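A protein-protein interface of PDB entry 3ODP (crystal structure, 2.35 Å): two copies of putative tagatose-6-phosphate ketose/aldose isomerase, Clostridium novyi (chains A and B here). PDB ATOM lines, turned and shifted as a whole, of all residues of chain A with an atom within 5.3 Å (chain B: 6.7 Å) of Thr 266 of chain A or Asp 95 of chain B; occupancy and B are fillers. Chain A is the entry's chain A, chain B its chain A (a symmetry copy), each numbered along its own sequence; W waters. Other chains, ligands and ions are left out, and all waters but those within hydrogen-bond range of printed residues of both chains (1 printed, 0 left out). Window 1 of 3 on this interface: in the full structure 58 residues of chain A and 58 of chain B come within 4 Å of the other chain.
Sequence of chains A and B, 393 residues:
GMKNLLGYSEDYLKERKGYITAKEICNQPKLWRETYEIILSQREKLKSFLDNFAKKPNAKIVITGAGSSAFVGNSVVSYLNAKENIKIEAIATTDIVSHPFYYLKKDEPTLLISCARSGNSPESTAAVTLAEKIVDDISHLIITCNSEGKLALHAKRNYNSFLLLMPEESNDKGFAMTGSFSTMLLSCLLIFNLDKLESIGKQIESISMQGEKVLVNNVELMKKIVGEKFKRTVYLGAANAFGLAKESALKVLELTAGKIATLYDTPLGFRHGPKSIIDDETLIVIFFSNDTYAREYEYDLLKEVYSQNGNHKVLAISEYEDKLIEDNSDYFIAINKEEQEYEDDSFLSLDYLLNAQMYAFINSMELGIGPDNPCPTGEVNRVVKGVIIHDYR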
ATOM      1  N   LEU A 236     -30.391  10.947  38.688  1.00  0.00           N
ATOM      2  CA  LEU A 236     -30.394  11.847  37.542  1.00  0.00           C
ATOM      3  C   LEU A 236     -29.230  12.839  37.655  1.00  0.00           C
ATOM      4  O   LEU A 236     -29.039  13.469  38.689  1.00  0.00           O
ATOM      5  CB  LEU A 236     -31.740  12.585  37.463  1.00  0.00           C
ATOM      6  CG  LEU A 236     -33.017  11.729  37.328  1.00  0.00           C
ATOM      7  CD1 LEU A 236     -34.303  12.566  37.336  1.00  0.00           C
ATOM      8  CD2 LEU A 236     -32.946  10.918  36.043  1.00  0.00           C
ATOM      9  N   GLY A 237     -28.437  12.943  36.593  1.00  0.00           N
ATOM     10  CA  GLY A 237     -27.300  13.863  36.549  1.00  0.00           C
ATOM     11  C   GLY A 237     -26.962  14.201  35.113  1.00  0.00           C
ATOM     12  O   GLY A 237     -26.849  13.309  34.271  1.00  0.00           O
ATOM     13  N   ALA A 238     -26.804  15.488  34.818  1.00  0.00           N
ATOM     14  CA  ALA A 238     -26.551  15.924  33.440  1.00  0.00           C
ATOM     15  C   ALA A 238     -25.048  16.014  33.188  1.00  0.00           C
ATOM     16  O   ALA A 238     -24.285  16.337  34.095  1.00  0.00           O
ATOM     17  CB  ALA A 238     -27.218  17.262  33.169  1.00  0.00           C
ATOM     18  N   ALA A 239     -24.643  15.699  31.962  1.00  0.00           N
ATOM     19  CA  ALA A 239     -23.265  15.831  31.512  1.00  0.00           C
ATOM     20  C   ALA A 239     -22.297  15.010  32.394  1.00  0.00           C
ATOM     21  O   ALA A 239     -22.386  13.777  32.419  1.00  0.00           O
ATOM     22  CB  ALA A 239     -22.875  17.323  31.443  1.00  0.00           C
ATOM     23  N   PHE A 242     -23.780  12.683  34.769  1.00  0.00           N
ATOM     24  CA  PHE A 242     -24.289  11.418  34.220  1.00  0.00           C
ATOM     25  C   PHE A 242     -23.448  10.245  34.713  1.00  0.00           C
ATOM     26  O   PHE A 242     -23.975   9.250  35.196  1.00  0.00           O
ATOM     27  CB  PHE A 242     -24.314  11.454  32.702  1.00  0.00           C
ATOM     28  CG  PHE A 242     -24.948  10.247  32.068  1.00  0.00           C
ATOM     29  CD1 PHE A 242     -26.297  10.008  32.198  1.00  0.00           C
ATOM     30  CD2 PHE A 242     -24.185   9.360  31.313  1.00  0.00           C
ATOM     31  CE1 PHE A 242     -26.897   8.900  31.580  1.00  0.00           C
ATOM     32  CE2 PHE A 242     -24.761   8.239  30.712  1.00  0.00           C
ATOM     33  CZ  PHE A 242     -26.121   8.010  30.842  1.00  0.00           C
ATOM     34  N   TYR A 264     -30.525   4.897  35.852  1.00  0.00           N
ATOM     35  CA  TYR A 264     -29.795   6.156  35.791  1.00  0.00           C
ATOM     36  C   TYR A 264     -30.154   6.849  34.481  1.00  0.00           C
ATOM     37  O   TYR A 264     -30.402   6.172  33.489  1.00  0.00           O
ATOM     38  CB  TYR A 264     -28.278   5.898  35.861  1.00  0.00           C
ATOM     39  CG  TYR A 264     -27.766   4.914  34.832  1.00  0.00           C
ATOM     40  CD1 TYR A 264     -27.722   3.547  35.107  1.00  0.00           C
ATOM     41  CD2 TYR A 264     -27.343   5.342  33.572  1.00  0.00           C
ATOM     42  CE1 TYR A 264     -27.268   2.631  34.156  1.00  0.00           C
ATOM     43  CE2 TYR A 264     -26.891   4.434  32.617  1.00  0.00           C
ATOM     44  CZ  TYR A 264     -26.853   3.085  32.915  1.00  0.00           C
ATOM     45  OH  TYR A 264     -26.404   2.186  31.974  1.00  0.00           O
ATOM     46  N   ASP A 265     -30.180   8.184  34.478  1.00  0.00           N
ATOM     47  CA  ASP A 265     -30.470   8.962  33.259  1.00  0.00           C
ATOM     48  C   ASP A 265     -30.094  10.424  33.494  1.00  0.00           C
ATOM     49  O   ASP A 265     -29.666  10.768  34.573  1.00  0.00           O
ATOM     50  CB  ASP A 265     -31.960   8.864  32.887  1.00  0.00           C
ATOM     51  CG  ASP A 265     -32.197   8.894  31.391  1.00  0.00           C
ATOM     52  OD1 ASP A 265     -31.728   9.840  30.726  1.00  0.00           O
ATOM     53  OD2 ASP A 265     -32.879   7.978  30.877  1.00  0.00           O
ATOM     54  N   THR A 266     -30.250  11.272  32.479  1.00  0.00           N
ATOM     55  CA  THR A 266     -30.104  12.719  32.650  1.00  0.00           C
ATOM     56  C   THR A 266     -31.496  13.277  32.943  1.00  0.00           C
ATOM     57  O   THR A 266     -32.495  12.573  32.732  1.00  0.00           O
ATOM     58  CB  THR A 266     -29.515  13.385  31.393  1.00  0.00           C
ATOM     59  OG1 THR A 266     -30.440  13.263  30.310  1.00  0.00           O
ATOM     60  CG2 THR A 266     -28.197  12.718  30.974  1.00  0.00           C
ATOM     61  N   PRO A 267     -31.584  14.528  33.441  1.00  0.00           N
ATOM     62  CA  PRO A 267     -32.942  14.987  33.757  1.00  0.00           C
ATOM     63  C   PRO A 267     -33.810  15.189  32.508  1.00  0.00           C
ATOM     64  O   PRO A 267     -34.875  14.594  32.401  1.00  0.00           O
ATOM     65  CB  PRO A 267     -32.709  16.292  34.530  1.00  0.00           C
ATOM     66  CG  PRO A 267     -31.320  16.149  35.112  1.00  0.00           C
ATOM     67  CD  PRO A 267     -30.557  15.417  34.012  1.00  0.00           C
ATOM     68  N   LEU A 268     -33.338  15.993  31.560  1.00  0.00           N
ATOM     69  CA  LEU A 268     -34.011  16.178  30.282  1.00  0.00           C
ATOM     70  C   LEU A 268     -34.366  14.846  29.615  1.00  0.00           C
ATOM     71  O   LEU A 268     -35.477  14.678  29.092  1.00  0.00           O
ATOM     72  CB  LEU A 268     -33.114  16.984  29.344  1.00  0.00           C
ATOM     73  CG  LEU A 268     -33.156  18.494  29.554  1.00  0.00           C
ATOM     74  CD1 LEU A 268     -32.149  19.152  28.634  1.00  0.00           C
ATOM     75  CD2 LEU A 268     -34.552  19.039  29.292  1.00  0.00           C
ATOM     76  N   GLY A 269     -33.413  13.913  29.648  1.00  0.00           N
ATOM     77  CA  GLY A 269     -33.549  12.607  29.005  1.00  0.00           C
ATOM     78  C   GLY A 269     -34.558  11.691  29.660  1.00  0.00           C
ATOM     79  O   GLY A 269     -35.171  10.866  28.988  1.00  0.00           O
ATOM     80  N   PHE A 270     -34.729  11.860  30.969  1.00  0.00           N
ATOM     81  CA  PHE A 270     -35.635  11.069  31.807  1.00  0.00           C
ATOM     82  C   PHE A 270     -37.070  11.080  31.291  1.00  0.00           C
ATOM     83  O   PHE A 270     -37.726  10.046  31.291  1.00  0.00           O
ATOM     84  CB  PHE A 270     -35.590  11.643  33.239  1.00  0.00           C
ATOM     85  CG  PHE A 270     -36.224  10.774  34.308  1.00  0.00           C
ATOM     86  CD1 PHE A 270     -35.943   9.415  34.401  1.00  0.00           C
ATOM     87  CD2 PHE A 270     -37.040  11.347  35.273  1.00  0.00           C
ATOM     88  CE1 PHE A 270     -36.498   8.634  35.418  1.00  0.00           C
ATOM     89  CE2 PHE A 270     -37.591  10.575  36.290  1.00  0.00           C
ATOM     90  CZ  PHE A 270     -37.326   9.214  36.357  1.00  0.00           C
ATOM     91  N   THR B  64     -27.881  12.957  16.650  1.00  0.00           N
ATOM     92  CA  THR B  64     -28.626  13.417  17.832  1.00  0.00           C
ATOM     93  C   THR B  64     -30.113  13.076  17.784  1.00  0.00           C
ATOM     94  O   THR B  64     -30.673  12.809  16.743  1.00  0.00           O
ATOM     95  CB  THR B  64     -28.438  14.941  18.072  1.00  0.00           C
ATOM     96  OG1 THR B  64     -28.854  15.291  19.403  1.00  0.00           O
ATOM     97  CG2 THR B  64     -29.197  15.777  17.039  1.00  0.00           C
ATOM     98  N   GLY B  65     -30.725  13.065  18.952  1.00  0.00           N
ATOM     99  CA  GLY B  65     -32.113  12.680  19.140  1.00  0.00           C
ATOM    100  C   GLY B  65     -32.401  12.614  20.637  1.00  0.00           C
ATOM    101  O   GLY B  65     -31.474  12.664  21.477  1.00  0.00           O
ATOM    102  N   ALA B  90     -22.531   9.790  18.809  1.00  0.00           N
ATOM    103  CA  ALA B  90     -23.912   9.884  19.283  1.00  0.00           C
ATOM    104  C   ALA B  90     -23.979  10.823  20.485  1.00  0.00           C
ATOM    105  O   ALA B  90     -23.441  10.513  21.543  1.00  0.00           O
ATOM    106  CB  ALA B  90     -24.425   8.517  19.690  1.00  0.00           C
ATOM    107  N   ILE B  91     -24.610  11.981  20.317  1.00  0.00           N
ATOM    108  CA  ILE B  91     -24.859  12.892  21.423  1.00  0.00           C
ATOM    109  C   ILE B  91     -26.335  13.249  21.402  1.00  0.00           C
ATOM    110  O   ILE B  91     -26.814  13.894  20.473  1.00  0.00           O
ATOM    111  CB  ILE B  91     -24.017  14.220  21.350  1.00  0.00           C
ATOM    112  CG1 ILE B  91     -22.567  13.973  20.924  1.00  0.00           C
ATOM    113  CG2 ILE B  91     -24.055  14.927  22.700  1.00  0.00           C
ATOM    114  CD1 ILE B  91     -21.774  15.256  20.733  1.00  0.00           C
ATOM    115  N   ALA B  92     -27.047  12.826  22.436  1.00  0.00           N
ATOM    116  CA  ALA B  92     -28.476  13.058  22.564  1.00  0.00           C
ATOM    117  C   ALA B  92     -28.815  14.541  22.603  1.00  0.00           C
ATOM    118  O   ALA B  92     -28.102  15.338  23.215  1.00  0.00           O
ATOM    119  CB  ALA B  92     -28.975  12.398  23.827  1.00  0.00           C
ATOM    120  N   THR B  93     -29.934  14.913  22.002  1.00  0.00           N
ATOM    121  CA  THR B  93     -30.427  16.288  22.134  1.00  0.00           C
ATOM    122  C   THR B  93     -30.609  16.655  23.587  1.00  0.00           C
ATOM    123  O   THR B  93     -30.377  17.798  23.959  1.00  0.00           O
ATOM    124  CB  THR B  93     -31.786  16.491  21.477  1.00  0.00           C
ATOM    125  OG1 THR B  93     -32.701  15.520  22.002  1.00  0.00           O
ATOM    126  CG2 THR B  93     -31.685  16.358  19.960  1.00  0.00           C
ATOM    127  N   THR B  94     -31.036  15.689  24.398  1.00  0.00           N
ATOM    128  CA  THR B  94     -31.230  15.902  25.832  1.00  0.00           C
ATOM    129  C   THR B  94     -29.917  16.108  26.625  1.00  0.00           C
ATOM    130  O   THR B  94     -29.957  16.296  27.836  1.00  0.00           O
ATOM    131  CB  THR B  94     -32.074  14.762  26.471  1.00  0.00           C
ATOM    132  OG1 THR B  94     -31.570  13.486  26.072  1.00  0.00           O
ATOM    133  CG2 THR B  94     -33.533  14.868  26.036  1.00  0.00           C
ATOM    134  N   ASP B  95     -28.771  16.056  25.937  1.00  0.00           N
ATOM    135  CA  ASP B  95     -27.455  16.438  26.483  1.00  0.00           C
ATOM    136  C   ASP B  95     -26.984  17.776  25.863  1.00  0.00           C
ATOM    137  O   ASP B  95     -26.518  18.670  26.572  1.00  0.00           O
ATOM    138  CB  ASP B  95     -26.411  15.341  26.190  1.00  0.00           C
ATOM    139  CG  ASP B  95     -26.771  13.984  26.806  1.00  0.00           C
ATOM    140  OD1 ASP B  95     -27.163  13.936  27.984  1.00  0.00           O
ATOM    141  OD2 ASP B  95     -26.642  12.948  26.115  1.00  0.00           O
ATOM    142  N   ILE B  96     -27.109  17.910  24.538  1.00  0.00           N
ATOM    143  CA  ILE B  96     -26.734  19.155  23.861  1.00  0.00           C
ATOM    144  C   ILE B  96     -27.454  20.358  24.465  1.00  0.00           C
ATOM    145  O   ILE B  96     -26.844  21.407  24.681  1.00  0.00           O
ATOM    146  CB  ILE B  96     -27.038  19.146  22.365  1.00  0.00           C
ATOM    147  CG1 ILE B  96     -26.231  18.078  21.642  1.00  0.00           C
ATOM    148  CG2 ILE B  96     -26.702  20.494  21.760  1.00  0.00           C
ATOM    149  CD1 ILE B  96     -26.599  17.925  20.159  1.00  0.00           C
ATOM    150  N   VAL B  97     -28.742  20.191  24.757  1.00  0.00           N
ATOM    151  CA  VAL B  97     -29.596  21.297  25.224  1.00  0.00           C
ATOM    152  C   VAL B  97     -29.277  21.795  26.629  1.00  0.00           C
ATOM    153  O   VAL B  97     -29.468  22.979  26.927  1.00  0.00           O
ATOM    154  CB  VAL B  97     -31.108  20.926  25.129  1.00  0.00           C
ATOM    155  CG1 VAL B  97     -31.971  21.933  25.883  1.00  0.00           C
ATOM    156  CG2 VAL B  97     -31.537  20.839  23.669  1.00  0.00           C
ATOM    157  N   SER B  98     -28.819  20.913  27.508  1.00  0.00           N
ATOM    158  CA  SER B  98     -28.432  21.364  28.845  1.00  0.00           C
ATOM    159  C   SER B  98     -27.005  21.928  28.855  1.00  0.00           C
ATOM    160  O   SER B  98     -26.717  22.835  29.626  1.00  0.00           O
ATOM    161  CB  SER B  98     -28.623  20.266  29.910  1.00  0.00           C
ATOM    162  OG  SER B  98     -27.932  19.070  29.610  1.00  0.00           O
ATOM    163  N   HIS B  99     -26.120  21.412  27.997  1.00  0.00           N
ATOM    164  CA  HIS B  99     -24.699  21.831  28.000  1.00  0.00           C
ATOM    165  C   HIS B  99     -24.106  21.999  26.624  1.00  0.00           C
ATOM    166  O   HIS B  99     -23.135  21.321  26.288  1.00  0.00           O
ATOM    167  CB  HIS B  99     -23.857  20.806  28.742  1.00  0.00           C
ATOM    168  CG  HIS B  99     -24.111  20.769  30.209  1.00  0.00           C
ATOM    169  ND1 HIS B  99     -25.253  20.225  30.755  1.00  0.00           N
ATOM    170  CD2 HIS B  99     -23.354  21.192  31.249  1.00  0.00           C
ATOM    171  CE1 HIS B  99     -25.180  20.308  32.070  1.00  0.00           C
ATOM    172  NE2 HIS B  99     -24.042  20.894  32.394  1.00  0.00           N
ATOM    173  N   PRO B 100     -24.652  22.931  25.824  1.00  0.00           N
ATOM    174  CA  PRO B 100     -24.209  23.054  24.438  1.00  0.00           C
ATOM    175  C   PRO B 100     -22.707  23.275  24.310  1.00  0.00           C
ATOM    176  O   PRO B 100     -22.106  22.815  23.339  1.00  0.00           O
ATOM    177  CB  PRO B 100     -24.973  24.288  23.942  1.00  0.00           C
ATOM    178  CG  PRO B 100     -25.291  25.035  25.162  1.00  0.00           C
ATOM    179  CD  PRO B 100     -25.581  24.009  26.182  1.00  0.00           C
ATOM    180  N   TYR B 103     -20.233  20.419  23.627  1.00  0.00           N
ATOM    181  CA  TYR B 103     -20.379  19.667  22.383  1.00  0.00           C
ATOM    182  C   TYR B 103     -20.354  20.472  21.078  1.00  0.00           C
ATOM    183  O   TYR B 103     -20.448  19.901  20.008  1.00  0.00           O
ATOM    184  CB  TYR B 103     -21.662  18.829  22.439  1.00  0.00           C
ATOM    185  CG  TYR B 103     -21.894  18.192  23.788  1.00  0.00           C
ATOM    186  CD1 TYR B 103     -21.023  17.233  24.280  1.00  0.00           C
ATOM    187  CD2 TYR B 103     -22.980  18.560  24.574  1.00  0.00           C
ATOM    188  CE1 TYR B 103     -21.227  16.660  25.517  1.00  0.00           C
ATOM    189  CE2 TYR B 103     -23.194  17.988  25.812  1.00  0.00           C
ATOM    190  CZ  TYR B 103     -22.314  17.038  26.275  1.00  0.00           C
ATOM    191  OH  TYR B 103     -22.522  16.478  27.508  1.00  0.00           O
HETATM  192  O   HOH W   1     -29.639  12.182  28.027  1.00  0.00           O
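Of the 12 printed residues of chain A, 5 touch a printed residue of chain B.
Printed residues of chain A that touch a printed residue of chain B: Ala 238, Ala 239, Thr 266, Leu 268 and Gly 269.
Hydrophobic or aromatic side chains of chain A that line the printed part of chain B: Ala 238, Ala 239 and Leu 268.
Printed residues of chain B that touch a printed residue of chain A: Thr 94, Asp 95, Val 97, Ser 98 and His 99.
Hydrophobic or aromatic side chains of chain B within 4 Å of the printed part of chain A: Val 97 and His 99.
Among the printed residues, no Asp or Glu carboxylate lies within 4 Å of a Lys or Arg side-chain nitrogen of the other chain.
Among the printed residues, merely in contact across the chains: Ala 238 of chain A with His 99 of chain B, Ala 239 of chain A with His 99 of chain B, Thr 266 of chain A with Thr 94 of chain B, Thr 266 of chain A with Asp 95 of chain B, Leu 268 of chain A with Thr 94 of chain B, Leu 268 of chain A with Val 97 of chain B, Leu 268 of chain A with Ser 98 of chain B and Gly 269 of chain A with Thr 94 of chain B.
Water W1 lies within hydrogen-bond range of the side-chain hydroxyl (OG1) of Thr 266 of chain A (2.6 Å), the side-chain carboxylate (OD1) of Asp 95 of chain B (3.0 Å) and the side-chain hydroxyl (OG1) of Thr 94 of chain B (3.0 Å).
No position is printed for both chains.
Of the 8 pairs that touch across the chains among the printed residues, none has its exchanged pair printed and touching as well.
Printed residues of chain B within 4 Å of Ala 238 of chain A: His 99 (3.8 Å).
Of the printed residues of chain B, Ala 239 of chain A touches His 99.
Thr 266 of chain A touches two residues of chain B.
Ala 90 of chain B touches none of the printed residues of chain A.
Asp 95 of chain B touches just one residue of chain A: Thr 266 (3.4 Å).
Of the printed residues of chain A, Val 97 of chain B touches Leu 268 (3.9 Å).
Printed residues of chain A within 4 Å of His 99 of chain B: Ala 238 and Ala 239.
The nearest residue of chain A that does not touch Asp 95 of chain B is Ala 239 of chain A (5.0 Å).
The side-chain hydroxyl (OG1) of Thr 266 of chain A is in hydrogen-bond range of the backbone NH (N) of Gly 269 of chain A.
The side-chain hydroxyl (OG) of Ser 98 of chain B is in hydrogen-bond range of the backbone carbonyl oxygen (O) of Asp 95 of chain B (3.4 Å).
OG of Ser 98 of chain B sits close to ND1 of His 99 of chain B, at 3.1 Å.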
